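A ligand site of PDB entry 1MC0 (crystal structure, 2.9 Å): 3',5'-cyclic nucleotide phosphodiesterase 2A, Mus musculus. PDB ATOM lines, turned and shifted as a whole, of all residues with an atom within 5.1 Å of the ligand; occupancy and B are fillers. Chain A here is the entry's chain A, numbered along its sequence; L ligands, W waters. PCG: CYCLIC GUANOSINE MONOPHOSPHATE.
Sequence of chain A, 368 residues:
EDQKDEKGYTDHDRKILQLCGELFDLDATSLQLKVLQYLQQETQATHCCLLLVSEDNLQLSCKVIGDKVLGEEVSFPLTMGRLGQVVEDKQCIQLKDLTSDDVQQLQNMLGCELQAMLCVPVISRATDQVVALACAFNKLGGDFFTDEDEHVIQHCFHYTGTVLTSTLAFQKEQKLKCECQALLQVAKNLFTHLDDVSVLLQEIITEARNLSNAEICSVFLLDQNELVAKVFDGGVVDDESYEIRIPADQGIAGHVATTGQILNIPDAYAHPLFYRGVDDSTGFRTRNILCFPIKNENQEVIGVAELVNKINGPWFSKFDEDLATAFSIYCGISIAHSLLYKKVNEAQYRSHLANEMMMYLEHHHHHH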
ATOM      1  N   ILE A 216      -7.745  34.183 -26.858  1.00  0.00           N
ATOM      2  CA  ILE A 216      -9.118  34.446 -27.255  1.00  0.00           C
ATOM      3  C   ILE A 216     -10.075  34.351 -26.081  1.00  0.00           C
ATOM      4  O   ILE A 216      -9.710  33.866 -25.017  1.00  0.00           O
ATOM      5  CB  ILE A 216      -9.626  33.459 -28.325  1.00  0.00           C
ATOM      6  CG1 ILE A 216      -9.613  32.044 -27.774  1.00  0.00           C
ATOM      7  CG2 ILE A 216      -8.757  33.541 -29.595  1.00  0.00           C
ATOM      8  CD1 ILE A 216      -9.908  31.023 -28.821  1.00  0.00           C
ATOM      9  N   CYS A 217     -11.297  34.814 -26.302  1.00  0.00           N
ATOM     10  CA  CYS A 217     -12.351  34.788 -25.300  1.00  0.00           C
ATOM     11  C   CYS A 217     -13.695  34.600 -26.005  1.00  0.00           C
ATOM     12  O   CYS A 217     -13.911  35.057 -27.118  1.00  0.00           O
ATOM     13  CB  CYS A 217     -12.365  36.094 -24.498  1.00  0.00           C
ATOM     14  SG  CYS A 217     -12.462  37.580 -25.517  1.00  0.00           S
ATOM     15  N   SER A 218     -14.604  33.921 -25.331  1.00  0.00           N
ATOM     16  CA  SER A 218     -15.897  33.678 -25.912  1.00  0.00           C
ATOM     17  C   SER A 218     -16.916  33.597 -24.818  1.00  0.00           C
ATOM     18  O   SER A 218     -16.609  33.163 -23.702  1.00  0.00           O
ATOM     19  CB  SER A 218     -15.893  32.363 -26.679  1.00  0.00           C
ATOM     20  OG  SER A 218     -15.917  31.276 -25.779  1.00  0.00           O
ATOM     21  N   PHE A 220     -20.887  32.180 -23.988  1.00  0.00           N
ATOM     22  CA  PHE A 220     -21.923  31.248 -24.436  1.00  0.00           C
ATOM     23  C   PHE A 220     -23.153  31.512 -23.587  1.00  0.00           C
ATOM     24  O   PHE A 220     -23.142  31.293 -22.373  1.00  0.00           O
ATOM     25  CB  PHE A 220     -21.497  29.783 -24.241  1.00  0.00           C
ATOM     26  CG  PHE A 220     -20.496  29.289 -25.259  1.00  0.00           C
ATOM     27  CD1 PHE A 220     -19.199  29.804 -25.289  1.00  0.00           C
ATOM     28  CD2 PHE A 220     -20.844  28.304 -26.164  1.00  0.00           C
ATOM     29  CE1 PHE A 220     -18.266  29.328 -26.218  1.00  0.00           C
ATOM     30  CE2 PHE A 220     -19.924  27.826 -27.095  1.00  0.00           C
ATOM     31  CZ  PHE A 220     -18.628  28.342 -27.124  1.00  0.00           C
ATOM     32  N   PHE A 232     -17.415  35.083 -29.869  1.00  0.00           N
ATOM     33  CA  PHE A 232     -16.503  34.025 -30.248  1.00  0.00           C
ATOM     34  C   PHE A 232     -15.258  34.652 -30.864  1.00  0.00           C
ATOM     35  O   PHE A 232     -15.345  35.460 -31.769  1.00  0.00           O
ATOM     36  CB  PHE A 232     -17.219  33.138 -31.267  1.00  0.00           C
ATOM     37  CG  PHE A 232     -16.653  31.773 -31.400  1.00  0.00           C
ATOM     38  CD1 PHE A 232     -16.914  30.795 -30.440  1.00  0.00           C
ATOM     39  CD2 PHE A 232     -15.861  31.438 -32.497  1.00  0.00           C
ATOM     40  CE1 PHE A 232     -16.408  29.503 -30.571  1.00  0.00           C
ATOM     41  CE2 PHE A 232     -15.353  30.161 -32.641  1.00  0.00           C
ATOM     42  CZ  PHE A 232     -15.623  29.188 -31.677  1.00  0.00           C
ATOM     43  N   ASP A 233     -14.098  34.252 -30.365  1.00  0.00           N
ATOM     44  CA  ASP A 233     -12.822  34.773 -30.842  1.00  0.00           C
ATOM     45  C   ASP A 233     -12.711  36.272 -30.627  1.00  0.00           C
ATOM     46  O   ASP A 233     -12.042  36.957 -31.388  1.00  0.00           O
ATOM     47  CB  ASP A 233     -12.606  34.435 -32.317  1.00  0.00           C
ATOM     48  CG  ASP A 233     -12.401  32.948 -32.555  1.00  0.00           C
ATOM     49  OD1 ASP A 233     -11.757  32.292 -31.707  1.00  0.00           O
ATOM     50  OD2 ASP A 233     -12.880  32.440 -33.583  1.00  0.00           O
ATOM     51  N   GLY A 234     -13.365  36.779 -29.598  1.00  0.00           N
ATOM     52  CA  GLY A 234     -13.277  38.190 -29.288  1.00  0.00           C
ATOM     53  C   GLY A 234     -14.291  39.082 -29.961  1.00  0.00           C
ATOM     54  O   GLY A 234     -14.448  40.229 -29.544  1.00  0.00           O
ATOM     55  N   ILE A 246     -24.001  24.201 -28.809  1.00  0.00           N
ATOM     56  CA  ILE A 246     -23.549  22.951 -28.220  1.00  0.00           C
ATOM     57  C   ILE A 246     -24.463  22.509 -27.071  1.00  0.00           C
ATOM     58  O   ILE A 246     -25.130  23.340 -26.461  1.00  0.00           O
ATOM     59  CB  ILE A 246     -22.098  23.120 -27.694  1.00  0.00           C
ATOM     60  CG1 ILE A 246     -21.162  22.183 -28.447  1.00  0.00           C
ATOM     61  CG2 ILE A 246     -22.020  22.863 -26.186  1.00  0.00           C
ATOM     62  CD1 ILE A 246     -19.716  22.355 -28.068  1.00  0.00           C
ATOM     63  N   GLN A 250     -22.378  19.476 -22.053  1.00  0.00           N
ATOM     64  CA  GLN A 250     -21.102  18.948 -22.532  1.00  0.00           C
ATOM     65  C   GLN A 250     -19.898  19.879 -22.374  1.00  0.00           C
ATOM     66  O   GLN A 250     -20.038  21.099 -22.250  1.00  0.00           O
ATOM     67  CB  GLN A 250     -21.242  18.540 -23.994  1.00  0.00           C
ATOM     68  CG  GLN A 250     -19.910  18.373 -24.695  1.00  0.00           C
ATOM     69  CD  GLN A 250     -20.084  18.111 -26.160  1.00  0.00           C
ATOM     70  OE1 GLN A 250     -20.342  16.982 -26.558  1.00  0.00           O
ATOM     71  NE2 GLN A 250     -19.971  19.163 -26.958  1.00  0.00           N
ATOM     72  N   GLY A 251     -18.721  19.267 -22.399  1.00  0.00           N
ATOM     73  CA  GLY A 251     -17.486  20.010 -22.269  1.00  0.00           C
ATOM     74  C   GLY A 251     -17.374  20.788 -20.982  1.00  0.00           C
ATOM     75  O   GLY A 251     -18.166  20.614 -20.049  1.00  0.00           O
ATOM     76  N   ILE A 252     -16.368  21.651 -20.945  1.00  0.00           N
ATOM     77  CA  ILE A 252     -16.100  22.506 -19.800  1.00  0.00           C
ATOM     78  C   ILE A 252     -17.155  23.603 -19.735  1.00  0.00           C
ATOM     79  O   ILE A 252     -17.618  23.960 -18.649  1.00  0.00           O
ATOM     80  CB  ILE A 252     -14.708  23.118 -19.941  1.00  0.00           C
ATOM     81  CG1 ILE A 252     -13.707  21.992 -20.208  1.00  0.00           C
ATOM     82  CG2 ILE A 252     -14.336  23.882 -18.680  1.00  0.00           C
ATOM     83  CD1 ILE A 252     -12.480  22.446 -20.929  1.00  0.00           C
ATOM     84  N   ALA A 253     -17.531  24.121 -20.898  1.00  0.00           N
ATOM     85  CA  ALA A 253     -18.560  25.163 -20.981  1.00  0.00           C
ATOM     86  C   ALA A 253     -19.811  24.632 -20.289  1.00  0.00           C
ATOM     87  O   ALA A 253     -20.342  25.259 -19.371  1.00  0.00           O
ATOM     88  CB  ALA A 253     -18.862  25.489 -22.429  1.00  0.00           C
ATOM     89  N   LEU A 273     -13.423  15.973 -19.248  1.00  0.00           N
ATOM     90  CA  LEU A 273     -14.589  16.706 -19.733  1.00  0.00           C
ATOM     91  C   LEU A 273     -14.418  17.566 -20.982  1.00  0.00           C
ATOM     92  O   LEU A 273     -15.396  18.056 -21.546  1.00  0.00           O
ATOM     93  CB  LEU A 273     -15.139  17.581 -18.599  1.00  0.00           C
ATOM     94  CG  LEU A 273     -15.555  16.873 -17.303  1.00  0.00           C
ATOM     95  CD1 LEU A 273     -15.924  17.887 -16.241  1.00  0.00           C
ATOM     96  CD2 LEU A 273     -16.730  15.952 -17.599  1.00  0.00           C
ATOM     97  N   PHE A 274     -13.183  17.755 -21.443  1.00  0.00           N
ATOM     98  CA  PHE A 274     -12.935  18.577 -22.609  1.00  0.00           C
ATOM     99  C   PHE A 274     -13.567  18.035 -23.896  1.00  0.00           C
ATOM    100  O   PHE A 274     -13.458  16.846 -24.197  1.00  0.00           O
ATOM    101  CB  PHE A 274     -11.428  18.742 -22.819  1.00  0.00           C
ATOM    102  CG  PHE A 274     -11.074  19.485 -24.079  1.00  0.00           C
ATOM    103  CD1 PHE A 274     -11.586  20.745 -24.331  1.00  0.00           C
ATOM    104  CD2 PHE A 274     -10.216  18.921 -25.007  1.00  0.00           C
ATOM    105  CE1 PHE A 274     -11.249  21.446 -25.490  1.00  0.00           C
ATOM    106  CE2 PHE A 274      -9.864  19.606 -26.168  1.00  0.00           C
ATOM    107  CZ  PHE A 274     -10.378  20.867 -26.403  1.00  0.00           C
ATOM    108  N   TYR A 275     -14.210  18.929 -24.643  1.00  0.00           N
ATOM    109  CA  TYR A 275     -14.843  18.573 -25.917  1.00  0.00           C
ATOM    110  C   TYR A 275     -14.010  19.132 -27.077  1.00  0.00           C
ATOM    111  O   TYR A 275     -14.052  20.334 -27.372  1.00  0.00           O
ATOM    112  CB  TYR A 275     -16.270  19.140 -25.992  1.00  0.00           C
ATOM    113  CG  TYR A 275     -16.893  19.008 -27.361  1.00  0.00           C
ATOM    114  CD1 TYR A 275     -17.308  17.766 -27.853  1.00  0.00           C
ATOM    115  CD2 TYR A 275     -17.049  20.116 -28.192  1.00  0.00           C
ATOM    116  CE1 TYR A 275     -17.871  17.647 -29.128  1.00  0.00           C
ATOM    117  CE2 TYR A 275     -17.605  20.009 -29.468  1.00  0.00           C
ATOM    118  CZ  TYR A 275     -18.010  18.771 -29.923  1.00  0.00           C
ATOM    119  OH  TYR A 275     -18.568  18.666 -31.182  1.00  0.00           O
ATOM    120  N   ARG A 276     -13.265  18.264 -27.737  1.00  0.00           N
ATOM    121  CA  ARG A 276     -12.412  18.669 -28.842  1.00  0.00           C
ATOM    122  C   ARG A 276     -13.150  19.089 -30.112  1.00  0.00           C
ATOM    123  O   ARG A 276     -12.574  19.739 -30.979  1.00  0.00           O
ATOM    124  CB  ARG A 276     -11.427  17.534 -29.151  1.00  0.00           C
ATOM    125  CG  ARG A 276     -12.096  16.175 -29.132  1.00  0.00           C
ATOM    126  CD  ARG A 276     -11.370  15.219 -28.223  1.00  0.00           C
ATOM    127  NE  ARG A 276     -10.424  14.381 -28.968  1.00  0.00           N
ATOM    128  CZ  ARG A 276      -9.551  13.562 -28.391  1.00  0.00           C
ATOM    129  NH1 ARG A 276      -9.500  13.456 -27.062  1.00  0.00           N
ATOM    130  NH2 ARG A 276      -8.743  12.832 -29.148  1.00  0.00           N
ATOM    131  N   VAL A 278     -15.258  21.459 -31.242  1.00  0.00           N
ATOM    132  CA  VAL A 278     -15.109  22.839 -31.699  1.00  0.00           C
ATOM    133  C   VAL A 278     -13.737  23.082 -32.315  1.00  0.00           C
ATOM    134  O   VAL A 278     -13.625  23.794 -33.314  1.00  0.00           O
ATOM    135  CB  VAL A 278     -15.324  23.822 -30.539  1.00  0.00           C
ATOM    136  CG1 VAL A 278     -15.432  25.234 -31.071  1.00  0.00           C
ATOM    137  CG2 VAL A 278     -16.567  23.420 -29.762  1.00  0.00           C
ATOM    138  N   ASP A 279     -12.695  22.502 -31.727  1.00  0.00           N
ATOM    139  CA  ASP A 279     -11.345  22.689 -32.256  1.00  0.00           C
ATOM    140  C   ASP A 279     -11.138  22.063 -33.634  1.00  0.00           C
ATOM    141  O   ASP A 279     -10.825  22.770 -34.592  1.00  0.00           O
ATOM    142  CB  ASP A 279     -10.297  22.124 -31.290  1.00  0.00           C
ATOM    143  CG  ASP A 279     -10.028  23.037 -30.111  1.00  0.00           C
ATOM    144  OD1 ASP A 279      -9.925  24.262 -30.310  1.00  0.00           O
ATOM    145  OD2 ASP A 279      -9.883  22.531 -28.982  1.00  0.00           O
ATOM    146  N   THR A 282     -12.975  24.235 -36.213  1.00  0.00           N
ATOM    147  CA  THR A 282     -12.390  25.521 -36.532  1.00  0.00           C
ATOM    148  C   THR A 282     -10.924  25.401 -36.931  1.00  0.00           C
ATOM    149  O   THR A 282     -10.380  26.280 -37.588  1.00  0.00           O
ATOM    150  CB  THR A 282     -12.410  26.464 -35.326  1.00  0.00           C
ATOM    151  OG1 THR A 282     -11.577  25.931 -34.295  1.00  0.00           O
ATOM    152  CG2 THR A 282     -13.829  26.614 -34.786  1.00  0.00           C
ATOM    153  N   PHE A 284      -8.536  25.123 -34.622  1.00  0.00           N
ATOM    154  CA  PHE A 284      -7.856  25.862 -33.562  1.00  0.00           C
ATOM    155  C   PHE A 284      -7.586  24.851 -32.448  1.00  0.00           C
ATOM    156  O   PHE A 284      -8.368  23.917 -32.246  1.00  0.00           O
ATOM    157  CB  PHE A 284      -8.768  26.983 -33.067  1.00  0.00           C
ATOM    158  CG  PHE A 284      -8.208  27.736 -31.894  1.00  0.00           C
ATOM    159  CD1 PHE A 284      -7.130  28.599 -32.047  1.00  0.00           C
ATOM    160  CD2 PHE A 284      -8.775  27.602 -30.629  1.00  0.00           C
ATOM    161  CE1 PHE A 284      -6.622  29.311 -30.969  1.00  0.00           C
ATOM    162  CE2 PHE A 284      -8.274  28.302 -29.550  1.00  0.00           C
ATOM    163  CZ  PHE A 284      -7.194  29.155 -29.714  1.00  0.00           C
ATOM    164  N   THR A 286      -7.023  24.184 -28.384  1.00  0.00           N
ATOM    165  CA  THR A 286      -7.166  24.701 -27.033  1.00  0.00           C
ATOM    166  C   THR A 286      -6.193  24.092 -26.017  1.00  0.00           C
ATOM    167  O   THR A 286      -6.247  22.903 -25.700  1.00  0.00           O
ATOM    168  CB  THR A 286      -8.589  24.464 -26.536  1.00  0.00           C
ATOM    169  OG1 THR A 286      -9.522  24.900 -27.533  1.00  0.00           O
ATOM    170  CG2 THR A 286      -8.832  25.242 -25.261  1.00  0.00           C
ATOM    171  N   ILE A 289      -8.039  26.480 -20.460  1.00  0.00           N
ATOM    172  CA  ILE A 289      -9.384  27.038 -20.448  1.00  0.00           C
ATOM    173  C   ILE A 289      -9.785  27.497 -19.062  1.00  0.00           C
ATOM    174  O   ILE A 289      -9.809  26.702 -18.119  1.00  0.00           O
ATOM    175  CB  ILE A 289     -10.411  26.009 -20.943  1.00  0.00           C
ATOM    176  CG1 ILE A 289     -10.170  25.707 -22.407  1.00  0.00           C
ATOM    177  CG2 ILE A 289     -11.818  26.554 -20.756  1.00  0.00           C
ATOM    178  CD1 ILE A 289     -11.195  24.793 -23.013  1.00  0.00           C
ATOM    179  N   GLU A 306     -15.535  32.014 -21.418  1.00  0.00           N
ATOM    180  CA  GLU A 306     -14.201  31.511 -21.233  1.00  0.00           C
ATOM    181  C   GLU A 306     -13.069  32.264 -21.882  1.00  0.00           C
ATOM    182  O   GLU A 306     -13.191  32.890 -22.934  1.00  0.00           O
ATOM    183  CB  GLU A 306     -14.103  30.020 -21.588  1.00  0.00           C
ATOM    184  CG  GLU A 306     -14.816  29.542 -22.811  1.00  0.00           C
ATOM    185  CD  GLU A 306     -14.992  28.027 -22.762  1.00  0.00           C
ATOM    186  OE1 GLU A 306     -15.565  27.527 -21.772  1.00  0.00           O
ATOM    187  OE2 GLU A 306     -14.555  27.321 -23.700  1.00  0.00           O
ATOM    188  N   VAL A 308      -9.345  31.661 -23.205  1.00  0.00           N
ATOM    189  CA  VAL A 308      -8.657  30.514 -23.776  1.00  0.00           C
ATOM    190  C   VAL A 308      -7.204  30.740 -24.163  1.00  0.00           C
ATOM    191  O   VAL A 308      -6.889  31.669 -24.888  1.00  0.00           O
ATOM    192  CB  VAL A 308      -9.412  30.010 -25.001  1.00  0.00           C
ATOM    193  CG1 VAL A 308      -8.606  28.928 -25.700  1.00  0.00           C
ATOM    194  CG2 VAL A 308     -10.754  29.466 -24.570  1.00  0.00           C
HETATM  195  PA  PCG L   1     -15.033  22.895 -24.517  1.00  0.00           P
HETATM  196  O1A PCG L   1     -14.689  21.731 -25.449  1.00  0.00           O
HETATM  197  O2A PCG L   1     -15.296  22.245 -23.145  1.00  0.00           O
HETATM  198  O5' PCG L   1     -16.272  23.528 -25.076  1.00  0.00           O
HETATM  199  C5' PCG L   1     -16.387  24.103 -26.425  1.00  0.00           C
HETATM  200  C4' PCG L   1     -15.018  24.541 -26.882  1.00  0.00           C
HETATM  201  O4' PCG L   1     -14.912  25.509 -27.969  1.00  0.00           O
HETATM  202  C3' PCG L   1     -14.261  25.107 -25.693  1.00  0.00           C
HETATM  203  O3' PCG L   1     -14.284  24.205 -24.480  1.00  0.00           O
HETATM  204  C2' PCG L   1     -13.025  25.412 -26.565  1.00  0.00           C
HETATM  205  O2' PCG L   1     -12.175  24.351 -27.028  1.00  0.00           O
HETATM  206  C1' PCG L   1     -13.621  26.120 -27.788  1.00  0.00           C
HETATM  207  N9  PCG L   1     -13.826  27.551 -27.538  1.00  0.00           N
HETATM  208  C8  PCG L   1     -14.339  28.359 -26.521  1.00  0.00           C
HETATM  209  N7  PCG L   1     -14.201  29.600 -26.969  1.00  0.00           N
HETATM  210  C5  PCG L   1     -13.674  29.721 -28.132  1.00  0.00           C
HETATM  211  C6  PCG L   1     -13.333  30.821 -29.009  1.00  0.00           C
HETATM  212  O6  PCG L   1     -13.506  32.073 -28.793  1.00  0.00           O
HETATM  213  N1  PCG L   1     -12.738  30.402 -30.230  1.00  0.00           N
HETATM  214  C2  PCG L   1     -12.486  29.075 -30.615  1.00  0.00           C
HETATM  215  N2  PCG L   1     -11.915  28.895 -31.826  1.00  0.00           N
HETATM  216  N3  PCG L   1     -12.783  28.003 -29.825  1.00  0.00           N
HETATM  217  C4  PCG L   1     -13.378  28.390 -28.594  1.00  0.00           C
HETATM  218  O   HOH W   1     -12.985  22.165 -28.773  1.00  0.00           O
HETATM  219  O   HOH W   2     -15.579  25.097 -22.436  1.00  0.00           O
HETATM  220  O   HOH W   3     -12.177  26.154 -31.595  1.00  0.00           O
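The backbone NH of Tyr 275 lies within hydrogen-bond range of an oxygen (O1A) of the ligand (3.0 Å). O of Tyr 275 sits close to O1A of the ligand, 2.5 Å away. N of Ile 252 lies within hydrogen-bond range of O2A of the ligand, at 2.5 Å. The backbone NH of Asp 233 is in hydrogen-bond range of an oxygen (O6) of the ligand, at 2.8 Å. The side-chain carboxylate of Asp 233 is in hydrogen-bond range of a nitrogen (N1) of the ligand (2.6 Å). The side-chain hydroxyl of Ser 218 is in hydrogen-bond range of a nitrogen (N7) of the ligand. O2' of the ligand lies within hydrogen-bond range of OG1 of Thr 286 (2.8 Å).
The backbone NH (N) of Asp 233 is in hydrogen-bond range of the backbone carbonyl oxygen (O) of Cys 217 (3.4 Å). The backbone carbonyl oxygen (O) of Ser 218 lies within hydrogen-bond range of the backbone NH (N) of Glu 306, at 2.8 Å. The side-chain carboxylate of Asp 279 sits at hydrogen-bond distance from the side-chain hydroxyl of Thr 286 (2.8 Å). The side-chain hydroxyl of Thr 282 sits at hydrogen-bond distance from the backbone carbonyl oxygen of Val 278 (3.1 Å). The backbone carbonyl oxygen of Ile 216 is in hydrogen-bond range of the backbone NH of Val 308, 2.9 Å away. The backbone carbonyl oxygen (O) of Cys 217 lies within hydrogen-bond range of the backbone NH (N) of Gly 234 (3.1 Å). The backbone NH of Phe 284 sits at hydrogen-bond distance from the backbone carbonyl oxygen of Asp 279. The backbone NH (N) of Phe 284 sits at hydrogen-bond distance from the side-chain hydroxyl (OG1) of Thr 282 (3.2 Å).
An oxygen (O6) of the ligand lies close to the backbone carbonyl oxygen of Cys 217, at 3.4 Å. O3' of the ligand lies close to OE2 of Glu 306 (3.2 Å). Ile 216 touches the ligand (CD1 to N1, 3.2 Å). CZ of Phe 232 touches C2 of the ligand, at 3.3 Å. CA of Gly 251 touches O2A of the ligand, 3.2 Å away. Ala 253 touches the ligand (N to O2A, 3.7 Å). CE1 of Phe 274 touches O2' of the ligand, 3.4 Å away. CB of Val 278 touches O4' of the ligand (3.1 Å). OD2 of Asp 279 touches O2' of the ligand (3.5 Å). OG1 of Thr 282 touches N2 of the ligand, 3.9 Å away. Phe 284 touches the ligand (CD2 to N2, 3.6 Å). Ile 289 touches the ligand. Hydrophobic or aromatic side chains within 4 Å of the ligand: Ile 216, Phe 232, Ile 252, Phe 274, Tyr 275, Val 278, Phe 284 and Ile 289. Within 4 Å of the ligand: Ile 216, Cys 217, Ser 218, Phe 232, Asp 233, Gly 251, Ile 252, Ala 253, Phe 274, Tyr 275, Val 278, Asp 279, Thr 282, Phe 284, Thr 286, Ile 289 and Glu 306. Along chain A the residues within 4 Å of the ligand span positions 216 to 306. The nearest printed residue that does not touch the ligand is Phe 220 (4.1 Å).
Water W2 lies within hydrogen-bond range of the side-chain carboxylate (OE1) of Glu 306, an oxygen (O3') of the ligand and the backbone NH (N) of Ala 253. Water W1 lies within hydrogen-bond range of O of Tyr 275, O2' of the ligand, N of Asp 279, O of Arg 276 and N of Val 278.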
